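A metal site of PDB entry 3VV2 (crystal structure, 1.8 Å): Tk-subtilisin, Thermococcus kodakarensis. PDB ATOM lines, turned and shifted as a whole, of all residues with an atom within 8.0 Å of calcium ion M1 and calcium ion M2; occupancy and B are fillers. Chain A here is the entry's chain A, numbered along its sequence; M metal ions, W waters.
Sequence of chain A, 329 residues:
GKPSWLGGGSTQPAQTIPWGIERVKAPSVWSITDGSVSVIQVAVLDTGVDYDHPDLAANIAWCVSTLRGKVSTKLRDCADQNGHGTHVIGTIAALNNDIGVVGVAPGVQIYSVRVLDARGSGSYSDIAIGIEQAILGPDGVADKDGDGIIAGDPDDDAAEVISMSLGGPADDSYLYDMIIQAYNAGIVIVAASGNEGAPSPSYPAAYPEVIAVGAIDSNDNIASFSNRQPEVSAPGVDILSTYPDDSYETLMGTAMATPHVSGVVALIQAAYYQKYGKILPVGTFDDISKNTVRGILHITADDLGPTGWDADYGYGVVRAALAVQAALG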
ATOM      1  N   VAL A 141      -5.892   3.574 -27.765  1.00  0.00           N
ATOM      2  CA  VAL A 141      -5.870   2.644 -28.884  1.00  0.00           C
ATOM      3  C   VAL A 141      -6.028   1.200 -28.327  1.00  0.00           C
ATOM      4  O   VAL A 141      -5.300   0.795 -27.402  1.00  0.00           O
ATOM      5  CB  VAL A 141      -4.550   2.807 -29.730  1.00  0.00           C
ATOM      6  CG1 VAL A 141      -4.564   1.921 -31.002  1.00  0.00           C
ATOM      7  CG2 VAL A 141      -4.290   4.311 -30.067  1.00  0.00           C
ATOM      8  N   ALA A 142      -6.996   0.489 -28.879  1.00  0.00           N
ATOM      9  CA  ALA A 142      -7.306  -0.862 -28.486  1.00  0.00           C
ATOM     10  C   ALA A 142      -6.128  -1.800 -28.803  1.00  0.00           C
ATOM     11  O   ALA A 142      -5.530  -2.390 -27.877  1.00  0.00           O
ATOM     12  CB  ALA A 142      -8.557  -1.291 -29.220  1.00  0.00           C
ATOM     13  N   ASP A 143      -5.703  -1.818 -30.076  1.00  0.00           N
ATOM     14  CA  ASP A 143      -4.707  -2.782 -30.567  1.00  0.00           C
ATOM     15  C   ASP A 143      -3.614  -2.060 -31.373  1.00  0.00           C
ATOM     16  O   ASP A 143      -3.703  -2.011 -32.632  1.00  0.00           O
ATOM     17  CB  ASP A 143      -5.449  -3.787 -31.473  1.00  0.00           C
ATOM     18  CG  ASP A 143      -4.522  -4.891 -32.039  1.00  0.00           C
ATOM     19  OD1 ASP A 143      -3.403  -5.024 -31.583  1.00  0.00           O
ATOM     20  OD2 ASP A 143      -4.955  -5.663 -32.871  1.00  0.00           O
ATOM     21  N   LYS A 144      -2.601  -1.518 -30.694  1.00  0.00           N
ATOM     22  CA  LYS A 144      -1.658  -0.590 -31.324  1.00  0.00           C
ATOM     23  C   LYS A 144      -0.804  -1.248 -32.428  1.00  0.00           C
ATOM     24  O   LYS A 144      -0.505  -0.604 -33.444  1.00  0.00           O
ATOM     25  CB  LYS A 144      -0.685  -0.102 -30.274  1.00  0.00           C
ATOM     26  CG  LYS A 144      -0.696   1.372 -30.083  1.00  0.00           C
ATOM     27  CD  LYS A 144       0.100   1.700 -28.816  1.00  0.00           C
ATOM     28  CE  LYS A 144       1.555   1.259 -28.933  1.00  0.00           C
ATOM     29  NZ  LYS A 144       2.045   0.804 -27.602  1.00  0.00           N
ATOM     30  N   ASP A 145      -0.457  -2.510 -32.259  1.00  0.00           N
ATOM     31  CA  ASP A 145       0.353  -3.186 -33.230  1.00  0.00           C
ATOM     32  C   ASP A 145      -0.425  -4.022 -34.248  1.00  0.00           C
ATOM     33  O   ASP A 145       0.152  -4.619 -35.123  1.00  0.00           O
ATOM     34  CB  ASP A 145       1.450  -3.981 -32.556  1.00  0.00           C
ATOM     35  CG  ASP A 145       0.916  -5.079 -31.670  1.00  0.00           C
ATOM     36  OD1 ASP A 145       1.740  -5.772 -31.057  1.00  0.00           O
ATOM     37  OD2 ASP A 145      -0.283  -5.327 -31.524  1.00  0.00           O
ATOM     38  N   GLY A 146      -1.741  -4.040 -34.140  1.00  0.00           N
ATOM     39  CA  GLY A 146      -2.586  -4.647 -35.185  1.00  0.00           C
ATOM     40  C   GLY A 146      -2.594  -6.142 -35.244  1.00  0.00           C
ATOM     41  O   GLY A 146      -3.084  -6.758 -36.243  1.00  0.00           O
ATOM     42  N   ASP A 147      -2.076  -6.768 -34.204  1.00  0.00           N
ATOM     43  CA  ASP A 147      -2.020  -8.260 -34.200  1.00  0.00           C
ATOM     44  C   ASP A 147      -3.258  -9.006 -33.684  1.00  0.00           C
ATOM     45  O   ASP A 147      -3.277 -10.239 -33.729  1.00  0.00           O
ATOM     46  CB  ASP A 147      -0.771  -8.804 -33.508  1.00  0.00           C
ATOM     47  CG  ASP A 147      -0.674  -8.362 -32.025  1.00  0.00           C
ATOM     48  OD1 ASP A 147      -1.638  -7.845 -31.379  1.00  0.00           O
ATOM     49  OD2 ASP A 147       0.417  -8.505 -31.506  1.00  0.00           O
ATOM     50  N   GLY A 148      -4.289  -8.300 -33.260  1.00  0.00           N
ATOM     51  CA  GLY A 148      -5.529  -8.994 -32.769  1.00  0.00           C
ATOM     52  C   GLY A 148      -5.432  -9.404 -31.308  1.00  0.00           C
ATOM     53  O   GLY A 148      -6.357  -9.860 -30.707  1.00  0.00           O
ATOM     54  N   ILE A 149      -4.254  -9.248 -30.693  1.00  0.00           N
ATOM     55  CA  ILE A 149      -4.121  -9.596 -29.306  1.00  0.00           C
ATOM     56  C   ILE A 149      -4.303  -8.261 -28.561  1.00  0.00           C
ATOM     57  O   ILE A 149      -3.620  -7.320 -28.885  1.00  0.00           O
ATOM     58  CB  ILE A 149      -2.692 -10.171 -29.014  1.00  0.00           C
ATOM     59  CG1 ILE A 149      -2.222 -11.134 -30.148  1.00  0.00           C
ATOM     60  CG2 ILE A 149      -2.610 -10.787 -27.591  1.00  0.00           C
ATOM     61  CD1 ILE A 149      -1.144 -12.138 -29.724  1.00  0.00           C
ATOM     62  N   ILE A 150      -5.216  -8.199 -27.632  1.00  0.00           N
ATOM     63  CA  ILE A 150      -5.442  -7.002 -26.861  1.00  0.00           C
ATOM     64  C   ILE A 150      -5.218  -7.282 -25.367  1.00  0.00           C
ATOM     65  O   ILE A 150      -4.243  -6.863 -24.813  1.00  0.00           O
ATOM     66  CB  ILE A 150      -6.817  -6.368 -27.165  1.00  0.00           C
ATOM     67  CG1 ILE A 150      -6.909  -5.951 -28.623  1.00  0.00           C
ATOM     68  CG2 ILE A 150      -7.045  -5.152 -26.293  1.00  0.00           C
ATOM     69  CD1 ILE A 150      -8.251  -6.001 -29.162  1.00  0.00           C
ATOM     70  N   ALA A 151      -6.079  -8.047 -24.731  1.00  0.00           N
ATOM     71  CA  ALA A 151      -5.851  -8.340 -23.326  1.00  0.00           C
ATOM     72  C   ALA A 151      -4.704  -9.333 -23.478  1.00  0.00           C
ATOM     73  O   ALA A 151      -4.694 -10.151 -24.429  1.00  0.00           O
ATOM     74  CB  ALA A 151      -7.111  -9.026 -22.711  1.00  0.00           C
ATOM     75  N   GLY A 152      -3.731  -9.233 -22.576  1.00  0.00           N
ATOM     76  CA  GLY A 152      -2.541 -10.101 -22.612  1.00  0.00           C
ATOM     77  C   GLY A 152      -1.409  -9.755 -23.569  1.00  0.00           C
ATOM     78  O   GLY A 152      -0.339 -10.409 -23.548  1.00  0.00           O
ATOM     79  N   ASP A 153      -1.607  -8.761 -24.421  1.00  0.00           N
ATOM     80  CA  ASP A 153      -0.524  -8.247 -25.241  1.00  0.00           C
ATOM     81  C   ASP A 153       0.309  -7.260 -24.462  1.00  0.00           C
ATOM     82  O   ASP A 153      -0.174  -6.210 -24.084  1.00  0.00           O
ATOM     83  CB  ASP A 153      -1.069  -7.612 -26.513  1.00  0.00           C
ATOM     84  CG  ASP A 153       0.015  -7.276 -27.515  1.00  0.00           C
ATOM     85  OD1 ASP A 153      -0.312  -7.062 -28.688  1.00  0.00           O
ATOM     86  OD2 ASP A 153       1.203  -7.206 -27.207  1.00  0.00           O
ATOM     87  N   PRO A 154       1.563  -7.587 -24.187  1.00  0.00           N
ATOM     88  CA  PRO A 154       2.328  -6.588 -23.415  1.00  0.00           C
ATOM     89  C   PRO A 154       2.579  -5.241 -24.101  1.00  0.00           C
ATOM     90  O   PRO A 154       2.930  -4.291 -23.388  1.00  0.00           O
ATOM     91  CB  PRO A 154       3.650  -7.281 -23.100  1.00  0.00           C
ATOM     92  CG  PRO A 154       3.768  -8.419 -24.142  1.00  0.00           C
ATOM     93  CD  PRO A 154       2.364  -8.775 -24.578  1.00  0.00           C
ATOM     94  N   ASP A 155       2.392  -5.173 -25.423  1.00  0.00           N
ATOM     95  CA  ASP A 155       2.566  -3.927 -26.225  1.00  0.00           C
ATOM     96  C   ASP A 155       1.314  -3.037 -26.058  1.00  0.00           C
ATOM     97  O   ASP A 155       1.350  -1.783 -26.223  1.00  0.00           O
ATOM     98  CB  ASP A 155       2.835  -4.198 -27.728  1.00  0.00           C
ATOM     99  CG  ASP A 155       3.093  -2.931 -28.478  1.00  0.00           C
ATOM    100  OD1 ASP A 155       3.976  -2.180 -28.023  1.00  0.00           O
ATOM    101  OD2 ASP A 155       2.390  -2.596 -29.457  1.00  0.00           O
ATOM    102  N   ASP A 156       0.213  -3.657 -25.682  1.00  0.00           N
ATOM    103  CA  ASP A 156      -0.970  -2.835 -25.363  1.00  0.00           C
ATOM    104  C   ASP A 156      -1.184  -2.557 -23.845  1.00  0.00           C
ATOM    105  O   ASP A 156      -0.487  -3.103 -22.990  1.00  0.00           O
ATOM    106  CB  ASP A 156      -2.240  -3.429 -25.965  1.00  0.00           C
ATOM    107  CG  ASP A 156      -2.267  -3.346 -27.501  1.00  0.00           C
ATOM    108  OD1 ASP A 156      -2.135  -2.224 -28.031  1.00  0.00           O
ATOM    109  OD2 ASP A 156      -2.428  -4.387 -28.165  1.00  0.00           O
ATOM    110  N   ASP A 157      -2.149  -1.707 -23.546  1.00  0.00           N
ATOM    111  CA  ASP A 157      -2.450  -1.344 -22.164  1.00  0.00           C
ATOM    112  C   ASP A 157      -3.901  -1.611 -21.824  1.00  0.00           C
ATOM    113  O   ASP A 157      -4.461  -0.984 -20.926  1.00  0.00           O
ATOM    114  CB  ASP A 157      -2.105   0.128 -21.915  1.00  0.00           C
ATOM    115  CG  ASP A 157      -2.786   1.061 -22.892  1.00  0.00           C
ATOM    116  OD1 ASP A 157      -2.513   2.280 -22.836  1.00  0.00           O
ATOM    117  OD2 ASP A 157      -3.582   0.579 -23.719  1.00  0.00           O
HETATM  118 CA    CA M   1      -1.901  -5.914 -29.969  1.00  0.00          CA
HETATM  119 CA    CA M   2       1.254  -7.458 -30.020  1.00  0.00          CA
HETATM  120  O   HOH W   1      -0.223  -3.759 -29.375  1.00  0.00           O
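The backbone NH of Asp 155 lies close to the side-chain carboxylate of Asp 153 (3.0 Å).
N of Gly 146 sits close to OD1 of Asp 143, at 3.2 Å.
The backbone NH (N) of Gly 148 is in hydrogen-bond range of the side-chain carboxylate (OD2) of Asp 143 (2.7 Å).
OD1 of Asp 156 lies within hydrogen-bond range of N of Lys 144 (2.8 Å).
Of the 17 residues printed, 6 come within 4 Å of calcium ion M1.
Within 4 Å of calcium ion M2: Asp 145, Asp 147 and Asp 153.
The nearest printed residue that does not touch calcium ion M2 is Asp 155 (4.3 Å).
Calcium ion M1 is bound by the side-chain carboxylate (OD2) of Asp 145, 2.3 Å away.
OD1 of Asp 153 is bound to calcium ion M1 (2.3 Å).
Calcium ion M1 is bound by the side-chain carboxylate (OD1) of Asp 143 (2.4 Å).
Calcium ion M1 is bound by OD1 of Asp 147, at 2.4 Å.
OD2 of Asp 156 binds calcium ion M1 (2.4 Å).
O of Ile 149 binds calcium ion M1, 2.5 Å away.
Calcium ion M1 is bound by water W1.
Calcium ion M1 has seven donor atoms within binding distance.
Calcium ion M2 is bound by the side-chain carboxylate (OD2) of Asp 147, the side-chain carboxylate (OD1) of Asp 145, the side-chain carboxylate (OD1) of Asp 153 and the side-chain carboxylate (OD2) of Asp 153.
Calcium ion M2 has four donor atoms within binding distance.
Slightly farther from calcium ion M2 lies OD2 of Asp 145 (3.0 Å).
Water W1 lies within hydrogen-bond range of the side-chain carboxylate of Asp 156 (2.8 Å), the side-chain carboxylate of Asp 155 (2.9 Å) and the backbone NH of Asp 145 (3.2 Å).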
